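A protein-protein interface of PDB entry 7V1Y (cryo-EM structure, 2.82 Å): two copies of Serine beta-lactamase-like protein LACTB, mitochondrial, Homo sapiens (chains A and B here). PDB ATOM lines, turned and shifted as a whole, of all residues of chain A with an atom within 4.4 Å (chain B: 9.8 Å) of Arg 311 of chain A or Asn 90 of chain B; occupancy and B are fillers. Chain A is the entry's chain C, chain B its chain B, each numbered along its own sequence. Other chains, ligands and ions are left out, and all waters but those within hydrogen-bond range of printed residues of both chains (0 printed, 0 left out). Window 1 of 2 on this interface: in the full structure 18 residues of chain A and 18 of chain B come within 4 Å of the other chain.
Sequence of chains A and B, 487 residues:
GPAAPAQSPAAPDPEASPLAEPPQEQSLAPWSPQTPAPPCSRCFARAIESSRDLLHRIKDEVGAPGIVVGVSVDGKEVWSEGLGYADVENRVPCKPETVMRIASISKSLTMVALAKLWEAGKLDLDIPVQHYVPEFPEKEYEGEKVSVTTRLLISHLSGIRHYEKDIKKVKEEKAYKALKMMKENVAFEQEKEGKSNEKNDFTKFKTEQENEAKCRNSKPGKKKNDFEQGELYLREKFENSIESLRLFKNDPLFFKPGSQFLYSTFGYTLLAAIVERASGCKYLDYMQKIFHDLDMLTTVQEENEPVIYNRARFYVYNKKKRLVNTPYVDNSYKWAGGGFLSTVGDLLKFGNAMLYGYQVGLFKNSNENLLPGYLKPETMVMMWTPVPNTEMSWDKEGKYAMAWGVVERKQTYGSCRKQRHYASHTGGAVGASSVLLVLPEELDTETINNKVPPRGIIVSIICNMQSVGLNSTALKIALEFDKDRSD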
ATOM      1  N   VAL A  92     -16.028   0.863 -25.326  1.00  0.00           N
ATOM      2  CA  VAL A  92     -15.859   0.506 -23.923  1.00  0.00           C
ATOM      3  C   VAL A  92     -17.159   0.844 -23.196  1.00  0.00           C
ATOM      4  O   VAL A  92     -17.506   2.027 -23.070  1.00  0.00           O
ATOM      5  CB  VAL A  92     -14.662   1.231 -23.293  1.00  0.00           C
ATOM      6  CG1 VAL A  92     -14.488   0.804 -21.845  1.00  0.00           C
ATOM      7  CG2 VAL A  92     -13.397   0.959 -24.088  1.00  0.00           C
ATOM      8  N   VAL A  99     -14.268   6.168 -14.321  1.00  0.00           N
ATOM      9  CA  VAL A  99     -13.715   7.364 -13.699  1.00  0.00           C
ATOM     10  C   VAL A  99     -13.986   8.541 -14.626  1.00  0.00           C
ATOM     11  O   VAL A  99     -13.501   8.569 -15.764  1.00  0.00           O
ATOM     12  CB  VAL A  99     -12.212   7.212 -13.421  1.00  0.00           C
ATOM     13  CG1 VAL A  99     -11.623   8.524 -12.943  1.00  0.00           C
ATOM     14  CG2 VAL A  99     -11.971   6.113 -12.400  1.00  0.00           C
ATOM     15  N   GLU A 302      -6.645  15.531 -11.952  1.00  0.00           N
ATOM     16  CA  GLU A 302      -6.590  15.470 -13.410  1.00  0.00           C
ATOM     17  C   GLU A 302      -5.147  15.575 -13.884  1.00  0.00           C
ATOM     18  O   GLU A 302      -4.550  16.654 -13.845  1.00  0.00           O
ATOM     19  CB  GLU A 302      -7.438  16.587 -14.012  1.00  0.00           C
ATOM     20  CG  GLU A 302      -7.704  16.456 -15.510  1.00  0.00           C
ATOM     21  CD  GLU A 302      -8.362  15.146 -15.890  1.00  0.00           C
ATOM     22  OE1 GLU A 302      -8.139  14.675 -17.025  1.00  0.00           O
ATOM     23  OE2 GLU A 302      -9.122  14.601 -15.067  1.00  0.00           O
ATOM     24  N   GLU A 303      -4.588  14.459 -14.346  1.00  0.00           N
ATOM     25  CA  GLU A 303      -3.244  14.445 -14.904  1.00  0.00           C
ATOM     26  C   GLU A 303      -3.209  13.514 -16.104  1.00  0.00           C
ATOM     27  O   GLU A 303      -3.992  12.565 -16.198  1.00  0.00           O
ATOM     28  CB  GLU A 303      -2.203  14.012 -13.865  1.00  0.00           C
ATOM     29  CG  GLU A 303      -1.695  15.149 -12.997  1.00  0.00           C
ATOM     30  CD  GLU A 303      -1.064  14.661 -11.711  1.00  0.00           C
ATOM     31  OE1 GLU A 303      -1.467  13.585 -11.221  1.00  0.00           O
ATOM     32  OE2 GLU A 303      -0.164  15.351 -11.189  1.00  0.00           O
ATOM     33  N   ASN A 304      -2.291  13.796 -17.025  1.00  0.00           N
ATOM     34  CA  ASN A 304      -2.173  13.052 -18.273  1.00  0.00           C
ATOM     35  C   ASN A 304      -1.098  11.974 -18.232  1.00  0.00           C
ATOM     36  O   ASN A 304      -1.326  10.864 -18.719  1.00  0.00           O
ATOM     37  CB  ASN A 304      -1.884  14.015 -19.431  1.00  0.00           C
ATOM     38  CG  ASN A 304      -1.668  13.295 -20.746  1.00  0.00           C
ATOM     39  OD1 ASN A 304      -0.575  13.329 -21.312  1.00  0.00           O
ATOM     40  ND2 ASN A 304      -2.710  12.641 -21.241  1.00  0.00           N
ATOM     41  N   PRO A 306       0.376  10.063 -15.673  1.00  0.00           N
ATOM     42  CA  PRO A 306       0.141   8.800 -14.963  1.00  0.00           C
ATOM     43  C   PRO A 306      -0.949   7.967 -15.617  1.00  0.00           C
ATOM     44  O   PRO A 306      -1.873   8.488 -16.247  1.00  0.00           O
ATOM     45  CB  PRO A 306      -0.278   9.252 -13.559  1.00  0.00           C
ATOM     46  CG  PRO A 306      -0.791  10.625 -13.747  1.00  0.00           C
ATOM     47  CD  PRO A 306       0.073  11.218 -14.810  1.00  0.00           C
ATOM     48  N   ILE A 308      -4.136   5.990 -15.345  1.00  0.00           N
ATOM     49  CA  ILE A 308      -5.318   5.911 -14.494  1.00  0.00           C
ATOM     50  C   ILE A 308      -6.289   4.938 -15.145  1.00  0.00           C
ATOM     51  O   ILE A 308      -6.769   5.185 -16.258  1.00  0.00           O
ATOM     52  CB  ILE A 308      -5.968   7.288 -14.289  1.00  0.00           C
ATOM     53  CG1 ILE A 308      -5.036   8.201 -13.493  1.00  0.00           C
ATOM     54  CG2 ILE A 308      -7.306   7.149 -13.586  1.00  0.00           C
ATOM     55  CD1 ILE A 308      -5.280   9.672 -13.723  1.00  0.00           C
ATOM     56  N   TYR A 309      -6.579   3.841 -14.454  1.00  0.00           N
ATOM     57  CA  TYR A 309      -7.425   2.803 -15.020  1.00  0.00           C
ATOM     58  C   TYR A 309      -8.881   3.246 -15.069  1.00  0.00           C
ATOM     59  O   TYR A 309      -9.354   4.008 -14.221  1.00  0.00           O
ATOM     60  CB  TYR A 309      -7.290   1.511 -14.218  1.00  0.00           C
ATOM     61  CG  TYR A 309      -5.901   0.921 -14.272  1.00  0.00           C
ATOM     62  CD1 TYR A 309      -5.466   0.228 -15.392  1.00  0.00           C
ATOM     63  CD2 TYR A 309      -5.021   1.067 -13.209  1.00  0.00           C
ATOM     64  CE1 TYR A 309      -4.197  -0.308 -15.453  1.00  0.00           C
ATOM     65  CE2 TYR A 309      -3.749   0.533 -13.260  1.00  0.00           C
ATOM     66  CZ  TYR A 309      -3.342  -0.153 -14.384  1.00  0.00           C
ATOM     67  OH  TYR A 309      -2.076  -0.687 -14.439  1.00  0.00           O
ATOM     68  N   ASN A 310      -9.590   2.759 -16.091  1.00  0.00           N
ATOM     69  CA  ASN A 310     -11.020   3.012 -16.282  1.00  0.00           C
ATOM     70  C   ASN A 310     -11.322   4.494 -16.486  1.00  0.00           C
ATOM     71  O   ASN A 310     -12.409   4.965 -16.145  1.00  0.00           O
ATOM     72  CB  ASN A 310     -11.844   2.454 -15.119  1.00  0.00           C
ATOM     73  CG  ASN A 310     -11.606   0.976 -14.893  1.00  0.00           C
ATOM     74  OD1 ASN A 310     -11.760   0.167 -15.805  1.00  0.00           O
ATOM     75  ND2 ASN A 310     -11.229   0.617 -13.674  1.00  0.00           N
ATOM     76  N   ARG A 311     -10.375   5.239 -17.047  1.00  0.00           N
ATOM     77  CA  ARG A 311     -10.604   6.645 -17.353  1.00  0.00           C
ATOM     78  C   ARG A 311     -11.414   6.768 -18.637  1.00  0.00           C
ATOM     79  O   ARG A 311     -11.099   6.124 -19.643  1.00  0.00           O
ATOM     80  CB  ARG A 311      -9.275   7.387 -17.483  1.00  0.00           C
ATOM     81  CG  ARG A 311      -9.383   8.740 -18.161  1.00  0.00           C
ATOM     82  CD  ARG A 311      -8.305   9.692 -17.680  1.00  0.00           C
ATOM     83  NE  ARG A 311      -6.967   9.148 -17.874  1.00  0.00           N
ATOM     84  CZ  ARG A 311      -5.845   9.806 -17.607  1.00  0.00           C
ATOM     85  NH1 ARG A 311      -5.865  11.042 -17.139  1.00  0.00           N
ATOM     86  NH2 ARG A 311      -4.677   9.205 -17.814  1.00  0.00           N
ATOM     87  N   ALA A 312     -12.457   7.594 -18.604  1.00  0.00           N
ATOM     88  CA  ALA A 312     -13.381   7.715 -19.717  1.00  0.00           C
ATOM     89  C   ALA A 312     -12.970   8.854 -20.649  1.00  0.00           C
ATOM     90  O   ALA A 312     -11.980   9.554 -20.427  1.00  0.00           O
ATOM     91  CB  ALA A 312     -14.805   7.918 -19.204  1.00  0.00           C
ATOM     92  N   TYR B  85      -2.130  -5.153 -25.404  1.00  0.00           N
ATOM     93  CA  TYR B  85      -3.248  -4.237 -25.239  1.00  0.00           C
ATOM     94  C   TYR B  85      -2.961  -2.934 -25.966  1.00  0.00           C
ATOM     95  O   TYR B  85      -1.911  -2.318 -25.757  1.00  0.00           O
ATOM     96  CB  TYR B  85      -3.518  -3.964 -23.756  1.00  0.00           C
ATOM     97  CG  TYR B  85      -3.972  -5.180 -22.986  1.00  0.00           C
ATOM     98  CD1 TYR B  85      -3.052  -6.031 -22.390  1.00  0.00           C
ATOM     99  CD2 TYR B  85      -5.321  -5.481 -22.856  1.00  0.00           C
ATOM    100  CE1 TYR B  85      -3.462  -7.146 -21.688  1.00  0.00           C
ATOM    101  CE2 TYR B  85      -5.740  -6.593 -22.155  1.00  0.00           C
ATOM    102  CZ  TYR B  85      -4.806  -7.422 -21.572  1.00  0.00           C
ATOM    103  OH  TYR B  85      -5.221  -8.531 -20.871  1.00  0.00           O
ATOM    104  N   ALA B  86      -3.896  -2.516 -26.823  1.00  0.00           N
ATOM    105  CA  ALA B  86      -3.779  -1.213 -27.466  1.00  0.00           C
ATOM    106  C   ALA B  86      -3.958  -0.086 -26.457  1.00  0.00           C
ATOM    107  O   ALA B  86      -3.289   0.950 -26.549  1.00  0.00           O
ATOM    108  CB  ALA B  86      -4.799  -1.092 -28.597  1.00  0.00           C
ATOM    109  N   ASP B  87      -4.858  -0.268 -25.494  1.00  0.00           N
ATOM    110  CA  ASP B  87      -5.075   0.685 -24.413  1.00  0.00           C
ATOM    111  C   ASP B  87      -5.005  -0.071 -23.096  1.00  0.00           C
ATOM    112  O   ASP B  87      -5.811  -0.975 -22.857  1.00  0.00           O
ATOM    113  CB  ASP B  87      -6.427   1.390 -24.563  1.00  0.00           C
ATOM    114  CG  ASP B  87      -6.607   2.527 -23.578  1.00  0.00           C
ATOM    115  OD1 ASP B  87      -5.629   2.885 -22.890  1.00  0.00           O
ATOM    116  OD2 ASP B  87      -7.730   3.064 -23.491  1.00  0.00           O
ATOM    117  N   VAL B  88      -4.045   0.296 -22.246  1.00  0.00           N
ATOM    118  CA  VAL B  88      -3.869  -0.402 -20.978  1.00  0.00           C
ATOM    119  C   VAL B  88      -4.767   0.141 -19.872  1.00  0.00           C
ATOM    120  O   VAL B  88      -4.994  -0.558 -18.874  1.00  0.00           O
ATOM    121  CB  VAL B  88      -2.398  -0.356 -20.521  1.00  0.00           C
ATOM    122  CG1 VAL B  88      -1.481  -0.819 -21.638  1.00  0.00           C
ATOM    123  CG2 VAL B  88      -2.023   1.040 -20.058  1.00  0.00           C
ATOM    124  N   GLU B  89      -5.281   1.365 -20.014  1.00  0.00           N
ATOM    125  CA  GLU B  89      -6.166   1.913 -18.993  1.00  0.00           C
ATOM    126  C   GLU B  89      -7.550   1.282 -19.059  1.00  0.00           C
ATOM    127  O   GLU B  89      -8.163   1.005 -18.022  1.00  0.00           O
ATOM    128  CB  GLU B  89      -6.260   3.431 -19.139  1.00  0.00           C
ATOM    129  CG  GLU B  89      -5.078   4.188 -18.557  1.00  0.00           C
ATOM    130  CD  GLU B  89      -5.221   5.690 -18.702  1.00  0.00           C
ATOM    131  OE1 GLU B  89      -5.990   6.133 -19.581  1.00  0.00           O
ATOM    132  OE2 GLU B  89      -4.567   6.430 -17.938  1.00  0.00           O
ATOM    133  N   ASN B  90      -8.059   1.050 -20.267  1.00  0.00           N
ATOM    134  CA  ASN B  90      -9.383   0.476 -20.459  1.00  0.00           C
ATOM    135  C   ASN B  90      -9.345  -0.988 -20.868  1.00  0.00           C
ATOM    136  O   ASN B  90     -10.404  -1.571 -21.121  1.00  0.00           O
ATOM    137  CB  ASN B  90     -10.160   1.288 -21.499  1.00  0.00           C
ATOM    138  CG  ASN B  90     -10.753   2.557 -20.922  1.00  0.00           C
ATOM    139  OD1 ASN B  90     -10.457   3.658 -21.382  1.00  0.00           O
ATOM    140  ND2 ASN B  90     -11.592   2.409 -19.905  1.00  0.00           N
ATOM    141  N   ARG B  91      -8.156  -1.591 -20.933  1.00  0.00           N
ATOM    142  CA  ARG B  91      -7.979  -3.011 -21.247  1.00  0.00           C
ATOM    143  C   ARG B  91      -8.598  -3.363 -22.602  1.00  0.00           C
ATOM    144  O   ARG B  91      -9.513  -4.179 -22.709  1.00  0.00           O
ATOM    145  CB  ARG B  91      -8.554  -3.896 -20.133  1.00  0.00           C
ATOM    146  CG  ARG B  91      -8.301  -3.396 -18.716  1.00  0.00           C
ATOM    147  CD  ARG B  91      -6.820  -3.216 -18.431  1.00  0.00           C
ATOM    148  NE  ARG B  91      -6.121  -4.491 -18.330  1.00  0.00           N
ATOM    149  CZ  ARG B  91      -4.817  -4.646 -18.508  1.00  0.00           C
ATOM    150  NH1 ARG B  91      -4.032  -3.622 -18.796  1.00  0.00           N
ATOM    151  NH2 ARG B  91      -4.287  -5.860 -18.396  1.00  0.00           N
ATOM    152  N   VAL B  92      -8.072  -2.728 -23.645  1.00  0.00           N
ATOM    153  CA  VAL B  92      -8.505  -2.947 -25.019  1.00  0.00           C
ATOM    154  C   VAL B  92      -7.438  -3.786 -25.717  1.00  0.00           C
ATOM    155  O   VAL B  92      -6.315  -3.307 -25.927  1.00  0.00           O
ATOM    156  CB  VAL B  92      -8.743  -1.621 -25.757  1.00  0.00           C
ATOM    157  CG1 VAL B  92      -9.236  -1.883 -27.170  1.00  0.00           C
ATOM    158  CG2 VAL B  92      -9.734  -0.759 -24.994  1.00  0.00           C
ATOM    159  N   PRO B  93      -7.733  -5.030 -26.092  1.00  0.00           N
ATOM    160  CA  PRO B  93      -6.711  -5.875 -26.721  1.00  0.00           C
ATOM    161  C   PRO B  93      -6.327  -5.380 -28.107  1.00  0.00           C
ATOM    162  O   PRO B  93      -7.116  -4.743 -28.808  1.00  0.00           O
ATOM    163  CB  PRO B  93      -7.382  -7.253 -26.795  1.00  0.00           C
ATOM    164  CG  PRO B  93      -8.576  -7.172 -25.893  1.00  0.00           C
ATOM    165  CD  PRO B  93      -9.004  -5.745 -25.903  1.00  0.00           C
ATOM    166  N   LYS B  95      -5.686  -5.739 -31.978  1.00  0.00           N
ATOM    167  CA  LYS B  95      -6.340  -6.470 -33.049  1.00  0.00           C
ATOM    168  C   LYS B  95      -5.798  -5.970 -34.376  1.00  0.00           C
ATOM    169  O   LYS B  95      -5.193  -4.894 -34.441  1.00  0.00           O
ATOM    170  CB  LYS B  95      -7.866  -6.296 -32.993  1.00  0.00           C
ATOM    171  CG  LYS B  95      -8.323  -4.869 -32.762  1.00  0.00           C
ATOM    172  CD  LYS B  95      -9.838  -4.780 -32.692  1.00  0.00           C
ATOM    173  CE  LYS B  95     -10.378  -5.505 -31.470  1.00  0.00           C
ATOM    174  NZ  LYS B  95      -9.973  -4.838 -30.202  1.00  0.00           N
ATOM    175  N   ARG B 311      -8.663   3.689 -32.484  1.00  0.00           N
ATOM    176  CA  ARG B 311      -7.429   4.437 -32.286  1.00  0.00           C
ATOM    177  C   ARG B 311      -6.766   4.004 -30.985  1.00  0.00           C
ATOM    178  O   ARG B 311      -7.424   3.919 -29.943  1.00  0.00           O
ATOM    179  CB  ARG B 311      -7.710   5.938 -32.273  1.00  0.00           C
ATOM    180  CG  ARG B 311      -6.580   6.777 -31.707  1.00  0.00           C
ATOM    181  CD  ARG B 311      -6.563   8.169 -32.309  1.00  0.00           C
ATOM    182  NE  ARG B 311      -7.832   8.862 -32.126  1.00  0.00           N
ATOM    183  CZ  ARG B 311      -8.059  10.116 -32.492  1.00  0.00           C
ATOM    184  NH1 ARG B 311      -7.118  10.851 -33.059  1.00  0.00           N
ATOM    185  NH2 ARG B 311      -9.261  10.645 -32.283  1.00  0.00           N
ATOM    186  N   ARG B 313      -3.420   3.929 -28.013  1.00  0.00           N
ATOM    187  CA  ARG B 313      -2.682   4.843 -27.156  1.00  0.00           C
ATOM    188  C   ARG B 313      -1.190   4.552 -27.255  1.00  0.00           C
ATOM    189  O   ARG B 313      -0.773   3.473 -27.684  1.00  0.00           O
ATOM    190  CB  ARG B 313      -3.148   4.730 -25.701  1.00  0.00           C
ATOM    191  CG  ARG B 313      -4.633   4.990 -25.503  1.00  0.00           C
ATOM    192  CD  ARG B 313      -4.937   6.477 -25.469  1.00  0.00           C
ATOM    193  NE  ARG B 313      -5.016   6.986 -24.106  1.00  0.00           N
ATOM    194  CZ  ARG B 313      -4.720   8.229 -23.751  1.00  0.00           C
ATOM    195  NH1 ARG B 313      -4.323   9.126 -24.638  1.00  0.00           N
ATOM    196  NH2 ARG B 313      -4.824   8.581 -22.472  1.00  0.00           N
ATOM    197  N   PHE B 314      -0.383   5.530 -26.855  1.00  0.00           N
ATOM    198  CA  PHE B 314       1.061   5.465 -27.017  1.00  0.00           C
ATOM    199  C   PHE B 314       1.743   5.749 -25.688  1.00  0.00           C
ATOM    200  O   PHE B 314       1.355   6.673 -24.967  1.00  0.00           O
ATOM    201  CB  PHE B 314       1.521   6.451 -28.094  1.00  0.00           C
ATOM    202  CG  PHE B 314       0.686   6.401 -29.339  1.00  0.00           C
ATOM    203  CD1 PHE B 314       0.829   5.362 -30.242  1.00  0.00           C
ATOM    204  CD2 PHE B 314      -0.264   7.375 -29.591  1.00  0.00           C
ATOM    205  CE1 PHE B 314       0.052   5.306 -31.381  1.00  0.00           C
ATOM    206  CE2 PHE B 314      -1.042   7.322 -30.731  1.00  0.00           C
ATOM    207  CZ  PHE B 314      -0.885   6.285 -31.626  1.00  0.00           C
ATOM    208  N   TYR B 315       2.770   4.961 -25.376  1.00  0.00           N
ATOM    209  CA  TYR B 315       3.362   4.931 -24.047  1.00  0.00           C
ATOM    210  C   TYR B 315       4.878   5.053 -24.132  1.00  0.00           C
ATOM    211  O   TYR B 315       5.483   4.897 -25.194  1.00  0.00           O
ATOM    212  CB  TYR B 315       2.984   3.644 -23.305  1.00  0.00           C
ATOM    213  CG  TYR B 315       1.500   3.372 -23.271  1.00  0.00           C
ATOM    214  CD1 TYR B 315       0.672   4.043 -22.383  1.00  0.00           C
ATOM    215  CD2 TYR B 315       0.927   2.446 -24.128  1.00  0.00           C
ATOM    216  CE1 TYR B 315      -0.683   3.799 -22.350  1.00  0.00           C
ATOM    217  CE2 TYR B 315      -0.428   2.194 -24.102  1.00  0.00           C
ATOM    218  CZ  TYR B 315      -1.227   2.872 -23.212  1.00  0.00           C
ATOM    219  OH  TYR B 315      -2.580   2.626 -23.182  1.00  0.00           O
ATOM    220  N   LEU B 323       5.646   2.497 -16.728  1.00  0.00           N
ATOM    221  CA  LEU B 323       4.947   2.861 -17.953  1.00  0.00           C
ATOM    222  C   LEU B 323       4.059   4.076 -17.717  1.00  0.00           C
ATOM    223  O   LEU B 323       3.262   4.103 -16.775  1.00  0.00           O
ATOM    224  CB  LEU B 323       4.113   1.683 -18.451  1.00  0.00           C
ATOM    225  CG  LEU B 323       3.599   1.754 -19.888  1.00  0.00           C
ATOM    226  CD1 LEU B 323       4.691   1.354 -20.866  1.00  0.00           C
ATOM    227  CD2 LEU B 323       2.374   0.874 -20.058  1.00  0.00           C
ATOM    228  N   VAL B 324       4.195   5.083 -18.580  1.00  0.00           N
ATOM    229  CA  VAL B 324       3.423   6.316 -18.490  1.00  0.00           C
ATOM    230  C   VAL B 324       2.916   6.683 -19.879  1.00  0.00           C
ATOM    231  O   VAL B 324       3.338   6.120 -20.890  1.00  0.00           O
ATOM    232  CB  VAL B 324       4.240   7.482 -17.893  1.00  0.00           C
ATOM    233  CG1 VAL B 324       4.570   7.212 -16.435  1.00  0.00           C
ATOM    234  CG2 VAL B 324       5.505   7.713 -18.698  1.00  0.00           C
ATOM    235  N   ASN B 325       1.993   7.639 -19.914  1.00  0.00           N
ATOM    236  CA  ASN B 325       1.456   8.139 -21.170  1.00  0.00           C
ATOM    237  C   ASN B 325       2.403   9.157 -21.792  1.00  0.00           C
ATOM    238  O   ASN B 325       3.089   9.907 -21.093  1.00  0.00           O
ATOM    239  CB  ASN B 325       0.085   8.783 -20.951  1.00  0.00           C
ATOM    240  CG  ASN B 325      -1.024   7.764 -20.810  1.00  0.00           C
ATOM    241  OD1 ASN B 325      -1.365   7.067 -21.762  1.00  0.00           O
ATOM    242  ND2 ASN B 325      -1.600   7.679 -19.618  1.00  0.00           N
ATOM    243  N   THR B 326       2.438   9.174 -23.120  1.00  0.00           N
ATOM    244  CA  THR B 326       3.220  10.177 -23.820  1.00  0.00           C
ATOM    245  C   THR B 326       2.491  11.520 -23.806  1.00  0.00           C
ATOM    246  O   THR B 326       1.257  11.564 -23.768  1.00  0.00           O
ATOM    247  CB  THR B 326       3.481   9.747 -25.260  1.00  0.00           C
ATOM    248  OG1 THR B 326       2.282   9.205 -25.825  1.00  0.00           O
ATOM    249  CG2 THR B 326       4.579   8.700 -25.310  1.00  0.00           C
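Among the printed residues, pairs that only touch across the chains: Val 92 of chain A with Asn 90 of chain B, Asn 304 of chain A with Thr 326 of chain B, Pro 306 of chain A with Glu 89 of chain B, Tyr 309 of chain A with Val 88 of chain B, Tyr 309 of chain A with Glu 89 of chain B, Asn 310 of chain A with Asn 90 of chain B and Arg 311 of chain A with Asn 325 of chain B.
Arg 311 of chain A touches just these residues of chain B: Glu 89, Asn 90 and Asn 325. No residue of chain B comes within 4 Å of Val 99 of chain A. Ile 308 of chain A touches just one residue of chain B: Glu 89 (2.7 Å). No residue of chain B comes within 4 Å of Ala 312 of chain A. Printed residues of chain A within 4 Å of Glu 89 of chain B: Pro 306, Ile 308, Tyr 309, Asn 310 and Arg 311. Of the printed residues of chain A, Thr 326 of chain B touches Asn 304. Printed residues of chain B within 4 Å of Val 92 of chain A: Asn 90 (3.8 Å). Arg 313 of chain B touches none of the printed residues of chain A. The nearest printed residue of chain B that does not touch Tyr 309 of chain A is Arg 91 of chain B (4.7 Å).
The backbone NH of Val 99 of chain A lies within hydrogen-bond range of the backbone carbonyl oxygen of Asn 310 of chain A. The guanidinium group (NH1) of Arg 311 of chain A is in hydrogen-bond range of the backbone carbonyl oxygen (O) of Glu 303 of chain A, at 2.6 Å. The backbone carbonyl oxygen (O) of Pro 306 of chain A sits at hydrogen-bond distance from the guanidinium group (NH2) of Arg 311 of chain A, at 3.3 Å. The guanidinium group (NH1) of Arg 91 of chain B lies within hydrogen-bond range of the backbone carbonyl oxygen (O) of Val 88 of chain B, at 3.2 Å. N of Val 88 of chain B is in hydrogen-bond range of OH of Tyr 315 of chain B (2.9 Å). The side-chain hydroxyl (OG1) of Thr 326 of chain B sits at hydrogen-bond distance from the backbone carbonyl oxygen (O) of Phe 314 of chain B (2.8 Å).
Along chain A the printed residues that touch a printed residue of chain B span positions 92 to 311. Among the printed residues, Asp or Glu carboxylates within 4 Å of a Lys or Arg side-chain nitrogen of the other chain: Arg 311 of chain A with Glu 89 of chain B (2.8 Å).
Positions printed for both chains: 92 and 311.
ND2 of Asn 325 of chain B sits at hydrogen-bond distance from O of Asn 304 of chain A (3.3 Å). ND2 of Asn 325 of chain B is in hydrogen-bond range of O of Pro 306 of chain A (3.5 Å). The side-chain carboxylate (OE2) of Glu 89 of chain B is in hydrogen-bond range of the backbone NH (N) of Ile 308 of chain A (2.7 Å). The backbone NH of Asn 310 of chain A lies within hydrogen-bond range of the backbone carbonyl oxygen of Glu 89 of chain B, 3.0 Å away. The guanidinium group of Arg 311 of chain A is in salt-bridge range of the side-chain carboxylate of Glu 89 of chain B (2.8 Å). The backbone carbonyl oxygen of Arg 311 of chain A lies close to the side-chain amide oxygen of Asn 90 of chain B, 3.1 Å away.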
